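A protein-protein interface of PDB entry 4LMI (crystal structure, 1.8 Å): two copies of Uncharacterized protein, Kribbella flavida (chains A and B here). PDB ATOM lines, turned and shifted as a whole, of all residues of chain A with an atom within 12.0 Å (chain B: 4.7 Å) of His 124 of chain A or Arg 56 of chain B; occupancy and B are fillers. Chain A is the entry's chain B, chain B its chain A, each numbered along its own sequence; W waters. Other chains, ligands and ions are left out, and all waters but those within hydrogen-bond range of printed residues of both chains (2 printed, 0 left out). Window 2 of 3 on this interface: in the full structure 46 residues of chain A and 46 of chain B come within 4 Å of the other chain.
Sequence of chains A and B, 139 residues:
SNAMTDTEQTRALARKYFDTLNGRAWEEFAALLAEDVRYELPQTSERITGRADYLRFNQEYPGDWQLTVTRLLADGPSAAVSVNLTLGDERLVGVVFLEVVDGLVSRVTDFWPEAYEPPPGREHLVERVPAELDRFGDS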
ATOM      1  N   PRO A 118      31.168 -25.318  22.083  1.00  0.00           N
ATOM      2  CA  PRO A 118      29.876 -24.841  22.576  1.00  0.00           C
ATOM      3  C   PRO A 118      28.871 -24.651  21.439  1.00  0.00           C
ATOM      4  O   PRO A 118      29.262 -24.246  20.340  1.00  0.00           O
ATOM      5  CB  PRO A 118      30.221 -23.493  23.212  1.00  0.00           C
ATOM      6  CG  PRO A 118      31.487 -23.059  22.550  1.00  0.00           C
ATOM      7  CD  PRO A 118      32.241 -24.325  22.284  1.00  0.00           C
ATOM      8  N   PRO A 119      27.586 -24.969  21.685  1.00  0.00           N
ATOM      9  CA  PRO A 119      26.550 -24.655  20.696  1.00  0.00           C
ATOM     10  C   PRO A 119      26.433 -23.142  20.473  1.00  0.00           C
ATOM     11  O   PRO A 119      26.691 -22.370  21.399  1.00  0.00           O
ATOM     12  CB  PRO A 119      25.265 -25.204  21.333  1.00  0.00           C
ATOM     13  CG  PRO A 119      25.586 -25.403  22.778  1.00  0.00           C
ATOM     14  CD  PRO A 119      27.048 -25.728  22.826  1.00  0.00           C
ATOM     15  N   PRO A 120      26.059 -22.717  19.249  1.00  0.00           N
ATOM     16  CA  PRO A 120      25.904 -21.287  18.951  1.00  0.00           C
ATOM     17  C   PRO A 120      24.727 -20.643  19.696  1.00  0.00           C
ATOM     18  O   PRO A 120      23.857 -21.351  20.206  1.00  0.00           O
ATOM     19  CB  PRO A 120      25.647 -21.271  17.439  1.00  0.00           C
ATOM     20  CG  PRO A 120      25.084 -22.618  17.138  1.00  0.00           C
ATOM     21  CD  PRO A 120      25.801 -23.554  18.062  1.00  0.00           C
ATOM     22  N   GLY A 121      24.719 -19.312  19.770  1.00  0.00           N
ATOM     23  CA  GLY A 121      23.571 -18.580  20.309  1.00  0.00           C
ATOM     24  C   GLY A 121      23.792 -17.795  21.589  1.00  0.00           C
ATOM     25  O   GLY A 121      22.910 -17.044  22.015  1.00  0.00           O
ATOM     26  N   ARG A 122      24.960 -17.959  22.208  1.00  0.00           N
ATOM     27  CA  ARG A 122      25.275 -17.254  23.455  1.00  0.00           C
ATOM     28  C   ARG A 122      26.605 -16.501  23.391  1.00  0.00           C
ATOM     29  O   ARG A 122      27.134 -16.074  24.422  1.00  0.00           O
ATOM     30  CB  ARG A 122      25.258 -18.222  24.641  1.00  0.00           C
ATOM     31  CG  ARG A 122      26.417 -19.206  24.667  1.00  0.00           C
ATOM     32  CD  ARG A 122      25.879 -20.595  24.889  1.00  0.00           C
ATOM     33  NE  ARG A 122      26.891 -21.569  25.279  1.00  0.00           N
ATOM     34  CZ  ARG A 122      26.609 -22.838  25.549  1.00  0.00           C
ATOM     35  NH1 ARG A 122      25.353 -23.260  25.463  1.00  0.00           N
ATOM     36  NH2 ARG A 122      27.569 -23.682  25.906  1.00  0.00           N
ATOM     37  N   GLU A 123      27.127 -16.333  22.176  1.00  0.00           N
ATOM     38  CA  GLU A 123      28.366 -15.590  21.941  1.00  0.00           C
ATOM     39  C   GLU A 123      28.356 -14.221  22.620  1.00  0.00           C
ATOM     40  O   GLU A 123      29.385 -13.762  23.115  1.00  0.00           O
ATOM     41  CB  GLU A 123      28.618 -15.422  20.439  1.00  0.00           C
ATOM     42  CG  GLU A 123      28.702 -16.724  19.649  1.00  0.00           C
ATOM     43  CD  GLU A 123      27.347 -17.244  19.185  1.00  0.00           C
ATOM     44  OE1 GLU A 123      26.306 -16.630  19.513  1.00  0.00           O
ATOM     45  OE2 GLU A 123      27.325 -18.277  18.484  1.00  0.00           O
ATOM     46  N   HIS A 124      27.185 -13.584  22.652  1.00  0.00           N
ATOM     47  CA  HIS A 124      27.028 -12.245  23.233  1.00  0.00           C
ATOM     48  C   HIS A 124      27.062 -12.227  24.742  1.00  0.00           C
ATOM     49  O   HIS A 124      27.201 -11.164  25.355  1.00  0.00           O
ATOM     50  CB  HIS A 124      25.757 -11.568  22.700  1.00  0.00           C
ATOM     51  CG  HIS A 124      24.468 -12.212  23.167  1.00  0.00           C
ATOM     52  ND1 HIS A 124      23.989 -13.351  22.628  1.00  0.00           N
ATOM     53  CD2 HIS A 124      23.549 -11.821  24.143  1.00  0.00           C
ATOM     54  CE1 HIS A 124      22.828 -13.680  23.233  1.00  0.00           C
ATOM     55  NE2 HIS A 124      22.560 -12.743  24.160  1.00  0.00           N
ATOM     56  N   LEU A 125      26.947 -13.401  25.356  1.00  0.00           N
ATOM     57  CA  LEU A 125      26.937 -13.512  26.816  1.00  0.00           C
ATOM     58  C   LEU A 125      28.218 -14.094  27.400  1.00  0.00           C
ATOM     59  O   LEU A 125      28.481 -13.939  28.595  1.00  0.00           O
ATOM     60  CB  LEU A 125      25.738 -14.342  27.284  1.00  0.00           C
ATOM     61  CG  LEU A 125      24.354 -13.726  27.055  1.00  0.00           C
ATOM     62  CD1 LEU A 125      23.267 -14.729  27.401  1.00  0.00           C
ATOM     63  CD2 LEU A 125      24.177 -12.437  27.849  1.00  0.00           C
ATOM     64  N   VAL A 126      29.006 -14.766  26.566  1.00  0.00           N
ATOM     65  CA  VAL A 126      30.196 -15.473  27.049  1.00  0.00           C
ATOM     66  C   VAL A 126      31.507 -14.749  26.757  1.00  0.00           C
ATOM     67  O   VAL A 126      31.621 -13.997  25.784  1.00  0.00           O
ATOM     68  CB  VAL A 126      30.284 -16.929  26.519  1.00  0.00           C
ATOM     69  CG1 VAL A 126      29.054 -17.721  26.924  1.00  0.00           C
ATOM     70  CG2 VAL A 126      30.477 -16.965  25.006  1.00  0.00           C
ATOM     71  N   GLU A 127      32.479 -14.972  27.632  1.00  0.00           N
ATOM     72  CA  GLU A 127      33.869 -14.652  27.358  1.00  0.00           C
ATOM     73  C   GLU A 127      34.587 -15.989  27.208  1.00  0.00           C
ATOM     74  O   GLU A 127      34.408 -16.889  28.036  1.00  0.00           O
ATOM     75  CB  GLU A 127      34.462 -13.840  28.510  1.00  0.00           C
ATOM     76  CG  GLU A 127      35.860 -13.301  28.252  1.00  0.00           C
ATOM     77  CD  GLU A 127      36.483 -12.668  29.485  1.00  0.00           C
ATOM     78  OE1 GLU A 127      36.379 -13.257  30.585  1.00  0.00           O
ATOM     79  OE2 GLU A 127      37.085 -11.581  29.352  1.00  0.00           O
ATOM     80  N   ARG A 128      35.370 -16.129  26.141  1.00  0.00           N
ATOM     81  CA  ARG A 128      36.156 -17.343  25.918  1.00  0.00           C
ATOM     82  C   ARG A 128      37.518 -17.227  26.597  1.00  0.00           C
ATOM     83  O   ARG A 128      38.357 -16.422  26.194  1.00  0.00           O
ATOM     84  CB  ARG A 128      36.323 -17.640  24.419  1.00  0.00           C
ATOM     85  CG  ARG A 128      35.028 -17.872  23.653  1.00  0.00           C
ATOM     86  CD  ARG A 128      34.153 -18.953  24.283  1.00  0.00           C
ATOM     87  NE  ARG A 128      34.706 -20.303  24.158  1.00  0.00           N
ATOM     88  CZ  ARG A 128      34.654 -21.041  23.050  1.00  0.00           C
ATOM     89  NH1 ARG A 128      34.098 -20.562  21.955  1.00  0.00           N
ATOM     90  NH2 ARG A 128      35.178 -22.256  23.039  1.00  0.00           N
ATOM     91  N   ALA B  52      22.974 -10.406  35.838  1.00  0.00           N
ATOM     92  CA  ALA B  52      22.165 -10.086  34.658  1.00  0.00           C
ATOM     93  C   ALA B  52      22.451 -11.018  33.479  1.00  0.00           C
ATOM     94  O   ALA B  52      21.522 -11.601  32.912  1.00  0.00           O
ATOM     95  CB  ALA B  52      22.339  -8.623  34.250  1.00  0.00           C
ATOM     96  N   ASP B  53      23.728 -11.166  33.123  1.00  0.00           N
ATOM     97  CA  ASP B  53      24.114 -12.012  31.988  1.00  0.00           C
ATOM     98  C   ASP B  53      23.828 -13.482  32.248  1.00  0.00           C
ATOM     99  O   ASP B  53      23.401 -14.203  31.342  1.00  0.00           O
ATOM    100  CB  ASP B  53      25.596 -11.856  31.650  1.00  0.00           C
ATOM    101  CG  ASP B  53      25.916 -10.547  30.967  1.00  0.00           C
ATOM    102  OD1 ASP B  53      24.998  -9.834  30.510  1.00  0.00           O
ATOM    103  OD2 ASP B  53      27.114 -10.234  30.881  1.00  0.00           O
ATOM    104  N   TYR B  54      24.073 -13.933  33.480  1.00  0.00           N
ATOM    105  CA  TYR B  54      23.805 -15.332  33.825  1.00  0.00           C
ATOM    106  C   TYR B  54      22.304 -15.653  33.799  1.00  0.00           C
ATOM    107  O   TYR B  54      21.901 -16.696  33.288  1.00  0.00           O
ATOM    108  CB  TYR B  54      24.445 -15.738  35.158  1.00  0.00           C
ATOM    109  CG  TYR B  54      24.360 -17.235  35.419  1.00  0.00           C
ATOM    110  CD1 TYR B  54      24.727 -18.154  34.432  1.00  0.00           C
ATOM    111  CD2 TYR B  54      23.914 -17.730  36.644  1.00  0.00           C
ATOM    112  CE1 TYR B  54      24.639 -19.518  34.651  1.00  0.00           C
ATOM    113  CE2 TYR B  54      23.829 -19.100  36.878  1.00  0.00           C
ATOM    114  CZ  TYR B  54      24.197 -19.986  35.881  1.00  0.00           C
ATOM    115  OH  TYR B  54      24.117 -21.340  36.094  1.00  0.00           O
ATOM    116  N   LEU B  55      21.485 -14.750  34.334  1.00  0.00           N
ATOM    117  CA  LEU B  55      20.031 -14.889  34.239  1.00  0.00           C
ATOM    118  C   LEU B  55      19.595 -14.981  32.774  1.00  0.00           C
ATOM    119  O   LEU B  55      18.801 -15.854  32.408  1.00  0.00           O
ATOM    120  CB  LEU B  55      19.327 -13.725  34.947  1.00  0.00           C
ATOM    121  CG  LEU B  55      17.797 -13.697  34.980  1.00  0.00           C
ATOM    122  CD1 LEU B  55      17.219 -14.932  35.661  1.00  0.00           C
ATOM    123  CD2 LEU B  55      17.316 -12.431  35.675  1.00  0.00           C
ATOM    124  N   ARG B  56      20.143 -14.094  31.944  1.00  0.00           N
ATOM    125  CA  ARG B  56      19.838 -14.056  30.512  1.00  0.00           C
ATOM    126  C   ARG B  56      20.205 -15.366  29.800  1.00  0.00           C
ATOM    127  O   ARG B  56      19.420 -15.880  28.998  1.00  0.00           O
ATOM    128  CB  ARG B  56      20.533 -12.852  29.857  1.00  0.00           C
ATOM    129  CG  ARG B  56      20.100 -12.569  28.429  1.00  0.00           C
ATOM    130  CD  ARG B  56      20.615 -11.221  27.944  1.00  0.00           C
ATOM    131  NE  ARG B  56      20.367 -11.030  26.515  1.00  0.00           N
ATOM    132  CZ  ARG B  56      20.952 -10.105  25.756  1.00  0.00           C
ATOM    133  NH1 ARG B  56      21.838  -9.266  26.278  1.00  0.00           N
ATOM    134  NH2 ARG B  56      20.651 -10.023  24.466  1.00  0.00           N
ATOM    135  N   PHE B  57      21.392 -15.896  30.099  1.00  0.00           N
ATOM    136  CA  PHE B  57      21.856 -17.181  29.551  1.00  0.00           C
ATOM    137  C   PHE B  57      20.840 -18.287  29.811  1.00  0.00           C
ATOM    138  O   PHE B  57      20.474 -19.036  28.899  1.00  0.00           O
ATOM    139  CB  PHE B  57      23.235 -17.536  30.141  1.00  0.00           C
ATOM    140  CG  PHE B  57      23.673 -18.966  29.909  1.00  0.00           C
ATOM    141  CD1 PHE B  57      24.066 -19.400  28.643  1.00  0.00           C
ATOM    142  CD2 PHE B  57      23.731 -19.868  30.969  1.00  0.00           C
ATOM    143  CE1 PHE B  57      24.483 -20.710  28.437  1.00  0.00           C
ATOM    144  CE2 PHE B  57      24.151 -21.180  30.768  1.00  0.00           C
ATOM    145  CZ  PHE B  57      24.526 -21.601  29.500  1.00  0.00           C
ATOM    146  N   ASN B  58      20.368 -18.369  31.053  1.00  0.00           N
ATOM    147  CA  ASN B  58      19.381 -19.379  31.432  1.00  0.00           C
ATOM    148  C   ASN B  58      18.008 -19.201  30.789  1.00  0.00           C
ATOM    149  O   ASN B  58      17.356 -20.191  30.436  1.00  0.00           O
ATOM    150  CB  ASN B  58      19.271 -19.468  32.954  1.00  0.00           C
ATOM    151  CG  ASN B  58      20.474 -20.144  33.570  1.00  0.00           C
ATOM    152  OD1 ASN B  58      20.653 -21.353  33.420  1.00  0.00           O
ATOM    153  ND2 ASN B  58      21.312 -19.370  34.255  1.00  0.00           N
ATOM    154  N   GLN B  59      17.588 -17.947  30.621  1.00  0.00           N
ATOM    155  CA  GLN B  59      16.291 -17.623  30.018  1.00  0.00           C
ATOM    156  C   GLN B  59      16.261 -17.835  28.504  1.00  0.00           C
ATOM    157  O   GLN B  59      15.238 -18.251  27.948  1.00  0.00           O
ATOM    158  CB  GLN B  59      15.885 -16.184  30.361  1.00  0.00           C
ATOM    159  CG  GLN B  59      15.494 -15.992  31.822  1.00  0.00           C
ATOM    160  CD  GLN B  59      15.307 -14.535  32.201  1.00  0.00           C
ATOM    161  OE1 GLN B  59      15.934 -13.644  31.630  1.00  0.00           O
ATOM    162  NE2 GLN B  59      14.448 -14.288  33.179  1.00  0.00           N
ATOM    163  N   GLU B  60      17.387 -17.560  27.849  1.00  0.00           N
ATOM    164  CA  GLU B  60      17.500 -17.683  26.396  1.00  0.00           C
ATOM    165  C   GLU B  60      17.816 -19.106  25.946  1.00  0.00           C
ATOM    166  O   GLU B  60      17.714 -19.414  24.760  1.00  0.00           O
ATOM    167  CB  GLU B  60      18.564 -16.724  25.854  1.00  0.00           C
ATOM    168  CG  GLU B  60      18.171 -15.258  25.934  1.00  0.00           C
ATOM    169  CD  GLU B  60      19.218 -14.325  25.353  1.00  0.00           C
ATOM    170  OE1 GLU B  60      20.288 -14.793  24.910  1.00  0.00           O
ATOM    171  OE2 GLU B  60      18.965 -13.104  25.340  1.00  0.00           O
HETATM  172  O   HOH W   1      29.196 -12.315  30.878  1.00  0.00           O
HETATM  173  O   HOH W   2      22.068 -16.888  25.001  1.00  0.00           O
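The guanidinium group (NH2) of Arg 56 of chain B sits at hydrogen-bond distance from a ring nitrogen (NE2) of His 124 of chain A (3.3 Å).
NE2 of His 124 of chain A is in hydrogen-bond range of OE1 of Glu 60 of chain B (3.2 Å).
The guanidinium group of Arg 56 of chain B lies within salt-bridge range of the side-chain carboxylate of Glu 60 of chain B (2.8 Å).
Among the printed residues, merely in contact across the chains: Arg 122 of chain A with Phe 57 of chain B, Leu 125 of chain A with Asp 53 of chain B, Leu 125 of chain A with Arg 56 of chain B, Leu 125 of chain A with Phe 57 of chain B and Leu 125 of chain A with Glu 60 of chain B.
Pro 120 of chain A touches none of the printed residues of chain B.
Of the printed residues of chain B, Arg 122 of chain A touches Phe 57 (3.8 Å).
Of chain B, only Arg 56 (3.3 Å) and Glu 60 (3.2 Å) come within 4 Å of His 124 of chain A.
Printed residues of chain B within 4 Å of Leu 125 of chain A: Asp 53, Arg 56, Phe 57 and Glu 60.
No residue of chain A comes within 4 Å of Ala 52 of chain B.
Printed residues of chain A within 4 Å of Asp 53 of chain B: Leu 125 (3.8 Å).
Tyr 54 of chain B touches none of the printed residues of chain A.
Of the printed residues of chain A, Arg 56 of chain B touches His 124 (3.3 Å) and Leu 125 (3.8 Å).
Of the 9 printed residues of chain B, 4 touch a printed residue of chain A.
Printed residues of chain B that touch a printed residue of chain A: Asp 53, Arg 56, Phe 57 and Glu 60.
Hydrophobic or aromatic side chains of chain B within 4 Å of the printed part of chain A: Phe 57.
Hydrophobic or aromatic side chains of chain A within 4 Å of the printed part of chain B: His 124 and Leu 125.
Along chain A the printed residues that touch a printed residue of chain B span positions 122 to 125.
Among the printed residues, no Asp or Glu carboxylate lies within 4 Å of a Lys or Arg side-chain nitrogen of the other chain.
No position is printed for both chains.
Water W2 bridges the side-chain carboxylate (OE1) of Glu 60 of chain B (2.8 Å) and the backbone carbonyl oxygen (O) of Gly 121 of chain A (3.1 Å).
Water W1 bridges the backbone carbonyl oxygen of Leu 125 of chain A (2.9 Å) and the side-chain carboxylate of Asp 53 of chain B (2.9 Å).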
